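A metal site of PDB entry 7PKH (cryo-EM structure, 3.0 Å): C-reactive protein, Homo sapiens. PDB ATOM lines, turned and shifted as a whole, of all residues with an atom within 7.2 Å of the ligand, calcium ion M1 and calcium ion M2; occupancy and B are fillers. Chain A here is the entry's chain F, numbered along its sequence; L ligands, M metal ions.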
ATOM      1  N   SER A  50      13.040 -12.984 -10.337  1.00  0.00           N
ATOM      2  CA  SER A  50      14.406 -12.533 -10.136  1.00  0.00           C
ATOM      3  C   SER A  50      14.852 -12.696  -8.685  1.00  0.00           C
ATOM      4  O   SER A  50      14.138 -12.298  -7.759  1.00  0.00           O
ATOM      5  CB  SER A  50      14.547 -11.083 -10.550  1.00  0.00           C
ATOM      6  OG  SER A  50      15.817 -10.575 -10.231  1.00  0.00           O
ATOM      7  N   SER A  53      19.476  -8.993  -9.300  1.00  0.00           N
ATOM      8  CA  SER A  53      19.555  -8.293 -10.579  1.00  0.00           C
ATOM      9  C   SER A  53      20.556  -7.150 -10.476  1.00  0.00           C
ATOM     10  O   SER A  53      20.393  -6.251  -9.657  1.00  0.00           O
ATOM     11  CB  SER A  53      18.185  -7.761 -10.986  1.00  0.00           C
ATOM     12  OG  SER A  53      18.310  -6.868 -12.065  1.00  0.00           O
ATOM     13  N   ALA A  55      22.371  -4.341 -12.941  1.00  0.00           N
ATOM     14  CA  ALA A  55      22.316  -3.666 -14.233  1.00  0.00           C
ATOM     15  C   ALA A  55      23.333  -2.538 -14.339  1.00  0.00           C
ATOM     16  O   ALA A  55      23.660  -1.879 -13.344  1.00  0.00           O
ATOM     17  CB  ALA A  55      20.925  -3.094 -14.495  1.00  0.00           C
ATOM     18  N   GLN A  59      23.384  -2.231 -20.084  1.00  0.00           N
ATOM     19  CA  GLN A  59      22.953  -3.627 -20.047  1.00  0.00           C
ATOM     20  C   GLN A  59      22.147  -3.858 -18.780  1.00  0.00           C
ATOM     21  O   GLN A  59      22.682  -3.773 -17.675  1.00  0.00           O
ATOM     22  CB  GLN A  59      24.155  -4.551 -20.107  1.00  0.00           C
ATOM     23  CG  GLN A  59      23.813  -6.009 -19.974  1.00  0.00           C
ATOM     24  CD  GLN A  59      22.738  -6.428 -20.931  1.00  0.00           C
ATOM     25  OE1 GLN A  59      21.578  -6.554 -20.562  1.00  0.00           O
ATOM     26  NE2 GLN A  59      23.110  -6.643 -22.189  1.00  0.00           N
ATOM     27  N   ASP A  60      20.855  -4.110 -18.953  1.00  0.00           N
ATOM     28  CA  ASP A  60      19.949  -4.331 -17.833  1.00  0.00           C
ATOM     29  C   ASP A  60      20.150  -5.677 -17.169  1.00  0.00           C
ATOM     30  O   ASP A  60      19.752  -5.846 -16.007  1.00  0.00           O
ATOM     31  CB  ASP A  60      18.501  -4.171 -18.309  1.00  0.00           C
ATOM     32  CG  ASP A  60      18.078  -5.269 -19.261  1.00  0.00           C
ATOM     33  OD1 ASP A  60      18.731  -5.436 -20.301  1.00  0.00           O
ATOM     34  OD2 ASP A  60      17.077  -5.949 -18.979  1.00  0.00           O
ATOM     35  N   ASN A  61      20.741  -6.644 -17.857  1.00  0.00           N
ATOM     36  CA  ASN A  61      20.975  -7.966 -17.297  1.00  0.00           C
ATOM     37  C   ASN A  61      22.461  -8.244 -17.205  1.00  0.00           C
ATOM     38  O   ASN A  61      22.930  -9.287 -17.671  1.00  0.00           O
ATOM     39  CB  ASN A  61      20.278  -9.032 -18.143  1.00  0.00           C
ATOM     40  CG  ASN A  61      18.785  -8.853 -18.188  1.00  0.00           C
ATOM     41  OD1 ASN A  61      18.224  -8.002 -17.509  1.00  0.00           O
ATOM     42  ND2 ASN A  61      18.119  -9.660 -18.997  1.00  0.00           N
ATOM     43  N   GLU A  62      23.212  -7.310 -16.617  1.00  0.00           N
ATOM     44  CA  GLU A  62      24.664  -7.438 -16.604  1.00  0.00           C
ATOM     45  C   GLU A  62      25.119  -8.544 -15.646  1.00  0.00           C
ATOM     46  O   GLU A  62      26.081  -9.261 -15.946  1.00  0.00           O
ATOM     47  CB  GLU A  62      25.277  -6.099 -16.237  1.00  0.00           C
ATOM     48  CG  GLU A  62      26.774  -6.093 -16.164  1.00  0.00           C
ATOM     49  CD  GLU A  62      27.412  -5.790 -17.502  1.00  0.00           C
ATOM     50  OE1 GLU A  62      26.779  -5.114 -18.330  1.00  0.00           O
ATOM     51  OE2 GLU A  62      28.551  -6.219 -17.724  1.00  0.00           O
ATOM     52  N   LEU A  64      22.376 -11.328 -13.662  1.00  0.00           N
ATOM     53  CA  LEU A  64      21.064 -11.680 -13.147  1.00  0.00           C
ATOM     54  C   LEU A  64      21.070 -13.132 -12.705  1.00  0.00           C
ATOM     55  O   LEU A  64      21.514 -14.001 -13.447  1.00  0.00           O
ATOM     56  CB  LEU A  64      20.000 -11.429 -14.212  1.00  0.00           C
ATOM     57  CG  LEU A  64      18.563 -11.829 -13.917  1.00  0.00           C
ATOM     58  CD1 LEU A  64      17.873 -10.786 -13.085  1.00  0.00           C
ATOM     59  CD2 LEU A  64      17.839 -12.020 -15.215  1.00  0.00           C
ATOM     60  N   PHE A  66      18.218 -15.791 -11.754  1.00  0.00           N
ATOM     61  CA  PHE A  66      16.793 -15.851 -12.017  1.00  0.00           C
ATOM     62  C   PHE A  66      16.331 -17.293 -11.913  1.00  0.00           C
ATOM     63  O   PHE A  66      16.932 -18.187 -12.511  1.00  0.00           O
ATOM     64  CB  PHE A  66      16.502 -15.282 -13.411  1.00  0.00           C
ATOM     65  CG  PHE A  66      15.078 -14.928 -13.646  1.00  0.00           C
ATOM     66  CD1 PHE A  66      14.632 -13.638 -13.488  1.00  0.00           C
ATOM     67  CD2 PHE A  66      14.179 -15.877 -14.075  1.00  0.00           C
ATOM     68  CE1 PHE A  66      13.321 -13.312 -13.723  1.00  0.00           C
ATOM     69  CE2 PHE A  66      12.868 -15.564 -14.298  1.00  0.00           C
ATOM     70  CZ  PHE A  66      12.443 -14.279 -14.127  1.00  0.00           C
ATOM     71  N   TRP A  67      15.276 -17.511 -11.136  1.00  0.00           N
ATOM     72  CA  TRP A  67      14.507 -18.751 -11.182  1.00  0.00           C
ATOM     73  C   TRP A  67      13.564 -18.751 -12.370  1.00  0.00           C
ATOM     74  O   TRP A  67      12.710 -17.874 -12.502  1.00  0.00           O
ATOM     75  CB  TRP A  67      13.715 -18.964  -9.897  1.00  0.00           C
ATOM     76  CG  TRP A  67      13.003 -20.249  -9.953  1.00  0.00           C
ATOM     77  CD1 TRP A  67      11.735 -20.459 -10.376  1.00  0.00           C
ATOM     78  CD2 TRP A  67      13.560 -21.536  -9.691  1.00  0.00           C
ATOM     79  NE1 TRP A  67      11.437 -21.789 -10.335  1.00  0.00           N
ATOM     80  CE2 TRP A  67      12.547 -22.472  -9.923  1.00  0.00           C
ATOM     81  CE3 TRP A  67      14.808 -21.985  -9.263  1.00  0.00           C
ATOM     82  CZ2 TRP A  67      12.740 -23.833  -9.744  1.00  0.00           C
ATOM     83  CZ3 TRP A  67      15.000 -23.332  -9.087  1.00  0.00           C
ATOM     84  CH2 TRP A  67      13.973 -24.241  -9.325  1.00  0.00           C
ATOM     85  N   SER A  68      13.695 -19.764 -13.222  1.00  0.00           N
ATOM     86  CA  SER A  68      12.860 -19.915 -14.410  1.00  0.00           C
ATOM     87  C   SER A  68      11.955 -21.119 -14.254  1.00  0.00           C
ATOM     88  O   SER A  68      12.422 -22.210 -13.939  1.00  0.00           O
ATOM     89  CB  SER A  68      13.719 -20.075 -15.656  1.00  0.00           C
ATOM     90  OG  SER A  68      14.190 -18.834 -16.121  1.00  0.00           O
ATOM     91  N   SER A  74      18.503 -19.615 -13.675  1.00  0.00           N
ATOM     92  CA  SER A  74      19.029 -18.905 -14.826  1.00  0.00           C
ATOM     93  C   SER A  74      20.125 -17.963 -14.368  1.00  0.00           C
ATOM     94  O   SER A  74      19.884 -17.072 -13.550  1.00  0.00           O
ATOM     95  CB  SER A  74      17.902 -18.146 -15.537  1.00  0.00           C
ATOM     96  OG  SER A  74      18.409 -17.199 -16.446  1.00  0.00           O
ATOM     97  N   THR A  76      22.892 -15.290 -15.843  1.00  0.00           N
ATOM     98  CA  THR A  76      23.298 -14.533 -17.008  1.00  0.00           C
ATOM     99  C   THR A  76      24.282 -13.433 -16.623  1.00  0.00           C
ATOM    100  O   THR A  76      24.106 -12.751 -15.613  1.00  0.00           O
ATOM    101  CB  THR A  76      22.114 -13.855 -17.687  1.00  0.00           C
ATOM    102  OG1 THR A  76      21.615 -12.817 -16.845  1.00  0.00           O
ATOM    103  CG2 THR A  76      21.002 -14.817 -17.898  1.00  0.00           C
ATOM    104  N   GLY A  79      23.908 -10.306 -20.396  1.00  0.00           N
ATOM    105  CA  GLY A  79      22.777 -10.771 -21.164  1.00  0.00           C
ATOM    106  C   GLY A  79      22.882 -12.151 -21.779  1.00  0.00           C
ATOM    107  O   GLY A  79      21.899 -12.613 -22.369  1.00  0.00           O
ATOM    108  N   GLU A  81      23.282 -16.277 -21.202  1.00  0.00           N
ATOM    109  CA  GLU A  81      22.634 -17.065 -20.164  1.00  0.00           C
ATOM    110  C   GLU A  81      23.085 -18.519 -20.233  1.00  0.00           C
ATOM    111  O   GLU A  81      23.403 -19.051 -21.294  1.00  0.00           O
ATOM    112  CB  GLU A  81      21.125 -17.015 -20.329  1.00  0.00           C
ATOM    113  CG  GLU A  81      20.360 -17.850 -19.349  1.00  0.00           C
ATOM    114  CD  GLU A  81      18.872 -17.711 -19.538  1.00  0.00           C
ATOM    115  OE1 GLU A  81      18.456 -16.850 -20.339  1.00  0.00           O
ATOM    116  OE2 GLU A  81      18.126 -18.467 -18.886  1.00  0.00           O
ATOM    117  N   LEU A  83      21.870 -22.348 -17.947  1.00  0.00           N
ATOM    118  CA  LEU A  83      20.871 -22.918 -17.044  1.00  0.00           C
ATOM    119  C   LEU A  83      21.479 -24.018 -16.183  1.00  0.00           C
ATOM    120  O   LEU A  83      22.307 -24.794 -16.650  1.00  0.00           O
ATOM    121  CB  LEU A  83      19.685 -23.486 -17.827  1.00  0.00           C
ATOM    122  CG  LEU A  83      18.674 -22.445 -18.329  1.00  0.00           C
ATOM    123  CD1 LEU A  83      17.867 -21.604 -17.334  1.00  0.00           C
ATOM    124  CD2 LEU A  83      18.740 -21.924 -19.761  1.00  0.00           C
ATOM    125  N   GLU A 138      13.060  -7.699 -10.990  1.00  0.00           N
ATOM    126  CA  GLU A 138      13.943  -7.784 -12.137  1.00  0.00           C
ATOM    127  C   GLU A 138      13.828  -6.446 -12.848  1.00  0.00           C
ATOM    128  O   GLU A 138      12.738  -5.902 -12.990  1.00  0.00           O
ATOM    129  CB  GLU A 138      13.534  -8.922 -13.071  1.00  0.00           C
ATOM    130  CG  GLU A 138      14.611  -9.349 -14.047  1.00  0.00           C
ATOM    131  CD  GLU A 138      14.706  -8.472 -15.256  1.00  0.00           C
ATOM    132  OE1 GLU A 138      13.665  -7.980 -15.733  1.00  0.00           O
ATOM    133  OE2 GLU A 138      15.835  -8.275 -15.752  1.00  0.00           O
ATOM    134  N   GLN A 139      14.964  -5.906 -13.272  1.00  0.00           N
ATOM    135  CA  GLN A 139      14.980  -4.581 -13.862  1.00  0.00           C
ATOM    136  C   GLN A 139      15.469  -4.598 -15.302  1.00  0.00           C
ATOM    137  O   GLN A 139      16.343  -5.379 -15.675  1.00  0.00           O
ATOM    138  CB  GLN A 139      15.824  -3.684 -12.959  1.00  0.00           C
ATOM    139  CG  GLN A 139      17.305  -3.768 -13.146  1.00  0.00           C
ATOM    140  CD  GLN A 139      18.026  -2.892 -12.153  1.00  0.00           C
ATOM    141  OE1 GLN A 139      17.463  -1.933 -11.635  1.00  0.00           O
ATOM    142  NE2 GLN A 139      19.256  -3.227 -11.848  1.00  0.00           N
ATOM    143  N   ASP A 140      14.876  -3.703 -16.106  1.00  0.00           N
ATOM    144  CA  ASP A 140      15.088  -3.655 -17.539  1.00  0.00           C
ATOM    145  C   ASP A 140      15.623  -2.323 -18.018  1.00  0.00           C
ATOM    146  O   ASP A 140      15.938  -2.188 -19.207  1.00  0.00           O
ATOM    147  CB  ASP A 140      13.792  -3.981 -18.288  1.00  0.00           C
ATOM    148  CG  ASP A 140      13.302  -5.386 -18.019  1.00  0.00           C
ATOM    149  OD1 ASP A 140      12.104  -5.558 -17.744  1.00  0.00           O
ATOM    150  OD2 ASP A 140      14.115  -6.320 -18.083  1.00  0.00           O
ATOM    151  N   SER A 141      15.725  -1.328 -17.153  1.00  0.00           N
ATOM    152  CA  SER A 141      16.534  -0.151 -17.379  1.00  0.00           C
ATOM    153  C   SER A 141      17.322   0.128 -16.114  1.00  0.00           C
ATOM    154  O   SER A 141      17.075  -0.476 -15.062  1.00  0.00           O
ATOM    155  CB  SER A 141      15.686   1.070 -17.764  1.00  0.00           C
ATOM    156  OG  SER A 141      14.887   1.488 -16.682  1.00  0.00           O
ATOM    157  N   GLY A 144      15.109   0.692 -13.167  1.00  0.00           N
ATOM    158  CA  GLY A 144      13.670   0.529 -13.239  1.00  0.00           C
ATOM    159  C   GLY A 144      13.153  -0.276 -14.399  1.00  0.00           C
ATOM    160  O   GLY A 144      13.851  -1.105 -14.964  1.00  0.00           O
ATOM    161  N   ASN A 145      11.906  -0.005 -14.785  1.00  0.00           N
ATOM    162  CA  ASN A 145      11.086  -0.888 -15.608  1.00  0.00           C
ATOM    163  C   ASN A 145      11.030  -2.301 -15.034  1.00  0.00           C
ATOM    164  O   ASN A 145      11.545  -3.260 -15.594  1.00  0.00           O
ATOM    165  CB  ASN A 145      11.611  -0.925 -17.043  1.00  0.00           C
ATOM    166  CG  ASN A 145      11.509   0.405 -17.721  1.00  0.00           C
ATOM    167  OD1 ASN A 145      12.499   1.112 -17.886  1.00  0.00           O
ATOM    168  ND2 ASN A 145      10.297   0.766 -18.121  1.00  0.00           N
ATOM    169  N   PHE A 146      10.368  -2.393 -13.877  1.00  0.00           N
ATOM    170  CA  PHE A 146      10.145  -3.671 -13.222  1.00  0.00           C
ATOM    171  C   PHE A 146       8.923  -4.361 -13.802  1.00  0.00           C
ATOM    172  O   PHE A 146       8.002  -3.723 -14.310  1.00  0.00           O
ATOM    173  CB  PHE A 146       9.990  -3.471 -11.729  1.00  0.00           C
ATOM    174  CG  PHE A 146      11.081  -2.646 -11.118  1.00  0.00           C
ATOM    175  CD1 PHE A 146      12.401  -3.005 -11.273  1.00  0.00           C
ATOM    176  CD2 PHE A 146      10.777  -1.521 -10.395  1.00  0.00           C
ATOM    177  CE1 PHE A 146      13.396  -2.250 -10.724  1.00  0.00           C
ATOM    178  CE2 PHE A 146      11.779  -0.756  -9.838  1.00  0.00           C
ATOM    179  CZ  PHE A 146      13.092  -1.124 -10.002  1.00  0.00           C
ATOM    180  N   GLU A 147       8.907  -5.693 -13.698  1.00  0.00           N
ATOM    181  CA  GLU A 147       7.772  -6.506 -14.120  1.00  0.00           C
ATOM    182  C   GLU A 147       7.238  -7.258 -12.921  1.00  0.00           C
ATOM    183  O   GLU A 147       7.971  -8.016 -12.278  1.00  0.00           O
ATOM    184  CB  GLU A 147       8.196  -7.488 -15.208  1.00  0.00           C
ATOM    185  CG  GLU A 147       8.160  -6.901 -16.595  1.00  0.00           C
ATOM    186  CD  GLU A 147       8.321  -7.933 -17.675  1.00  0.00           C
ATOM    187  OE1 GLU A 147       7.749  -9.033 -17.545  1.00  0.00           O
ATOM    188  OE2 GLU A 147       9.037  -7.646 -18.662  1.00  0.00           O
ATOM    189  N   SER A 149       5.299  -9.770 -12.740  1.00  0.00           N
ATOM    190  CA  SER A 149       5.422 -11.208 -12.916  1.00  0.00           C
ATOM    191  C   SER A 149       6.826 -11.736 -12.651  1.00  0.00           C
ATOM    192  O   SER A 149       6.982 -12.946 -12.471  1.00  0.00           O
ATOM    193  CB  SER A 149       5.003 -11.605 -14.328  1.00  0.00           C
ATOM    194  OG  SER A 149       5.870 -11.039 -15.286  1.00  0.00           O
ATOM    195  N   GLN A 150       7.834 -10.878 -12.619  1.00  0.00           N
ATOM    196  CA  GLN A 150       9.199 -11.289 -12.295  1.00  0.00           C
ATOM    197  C   GLN A 150       9.655 -10.888 -10.903  1.00  0.00           C
ATOM    198  O   GLN A 150      10.804 -11.137 -10.556  1.00  0.00           O
ATOM    199  CB  GLN A 150      10.154 -10.723 -13.341  1.00  0.00           C
ATOM    200  CG  GLN A 150       9.898 -11.250 -14.722  1.00  0.00           C
ATOM    201  CD  GLN A 150      10.852 -10.695 -15.746  1.00  0.00           C
ATOM    202  OE1 GLN A 150      11.309  -9.560 -15.634  1.00  0.00           O
ATOM    203  NE2 GLN A 150      11.136 -11.485 -16.763  1.00  0.00           N
HETATM  204  P1  LIG L   1      14.132  -9.876 -19.057  1.00  0.00           P
HETATM  205  O1  LIG L   1      12.678  -9.196 -18.995  1.00  0.00           O
HETATM  206  O2  LIG L   1      14.675  -9.850 -20.421  1.00  0.00           O
HETATM  207  O3  LIG L   1      15.030  -9.002 -18.045  1.00  0.00           O
HETATM  208  O4  LIG L   1      13.981 -11.386 -18.541  1.00  0.00           O
HETATM  209  C1  LIG L   1      15.151 -11.730 -17.800  1.00  0.00           C
HETATM  210  C2  LIG L   1      15.093 -13.184 -17.330  1.00  0.00           C
HETATM  211  N1  LIG L   1      15.316 -14.213 -18.358  1.00  0.00           N
HETATM  212  C3  LIG L   1      14.339 -14.094 -19.437  1.00  0.00           C
HETATM  213  C4  LIG L   1      15.166 -15.545 -17.762  1.00  0.00           C
HETATM  214  C5  LIG L   1      16.654 -14.108 -18.930  1.00  0.00           C
HETATM  215 CA    CA M   1      11.944  -7.857 -17.139  1.00  0.00          CA
HETATM  216 CA    CA M   2      16.095  -7.104 -17.453  1.00  0.00          CA
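The backbone NH (N) of Leu 64 is in hydrogen-bond range of the backbone carbonyl oxygen (O) of Thr 76, 3.0 Å away.
The backbone carbonyl oxygen (O) of Gln 150 sits at hydrogen-bond distance from the backbone NH (N) of Ser 50, at 2.9 Å.
The side-chain carboxylate of Asp 60 sits close to the side-chain amide oxygen of Gln 59 (3.1 Å).
O of Phe 66 is in hydrogen-bond range of N of Ser 74 (2.4 Å).
O of Asn 61 lies within hydrogen-bond range of N of Gly 79 (3.1 Å).
NE2 of Gln 139 sits close to N of Ala 55 (3.5 Å).
The backbone NH of Asn 61 lies within hydrogen-bond range of the side-chain amide oxygen of Gln 59 (2.8 Å).
The backbone carbonyl oxygen (O) of Asn 145 lies within hydrogen-bond range of the backbone NH (N) of Asp 140 (3.4 Å).
Leu 64 touches the ligand.
CD2 of Phe 66 touches C4 of the ligand (3.8 Å).
OG of Ser 68 touches C4 of the ligand, 3.8 Å away.
Ser 74 touches the ligand (OG to C4, 3.9 Å).
Glu 81 touches the ligand.
Glu 147 touches the ligand.
Hydrophobic or aromatic side chains that line the ligand: Leu 64 and Phe 66.
Within 4 Å of the ligand: Asp 60, Asn 61, Leu 64, Phe 66, Ser 68, Ser 74, Glu 81, Glu 138, Asp 140, Glu 147 and Gln 150.
Glu 147 touches calcium ion M1.
Four residues have an atom within 4 Å of calcium ion M1: Glu 138, Asp 140, Glu 147 and Gln 150.
Calcium ion M2 is bound by OE2 of Glu 138.
Calcium ion M2 is bound by OD2 of Asp 60.
Calcium ion M2 is bound by OD2 of Asp 140 (2.2 Å).
An oxygen (O3) of the ligand binds calcium ion M2, 2.3 Å away.
OD1 of Asn 61 is bound to calcium ion M2.
O of Gln 139 binds calcium ion M2 (2.5 Å).
Slightly farther from calcium ion M2 lies OE1 of Glu 138 (3.1 Å).
Calcium ion M1 is bound by the side-chain carboxylate (OE1) of Glu 138 (2.2 Å), the side-chain amide oxygen (OE1) of Gln 150 (2.4 Å), the side-chain carboxylate (OD1) of Asp 140 (2.4 Å), an oxygen (O1) of the ligand (2.4 Å) and the side-chain carboxylate (OD2) of Asp 140 (2.8 Å).
Calcium ion M1 has five donor atoms within binding distance.
Of the 26 residues printed, 5 come within 4 Å of calcium ion M2.
The nearest printed residue that does not touch calcium ion M2 is Leu 64 (5.7 Å).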
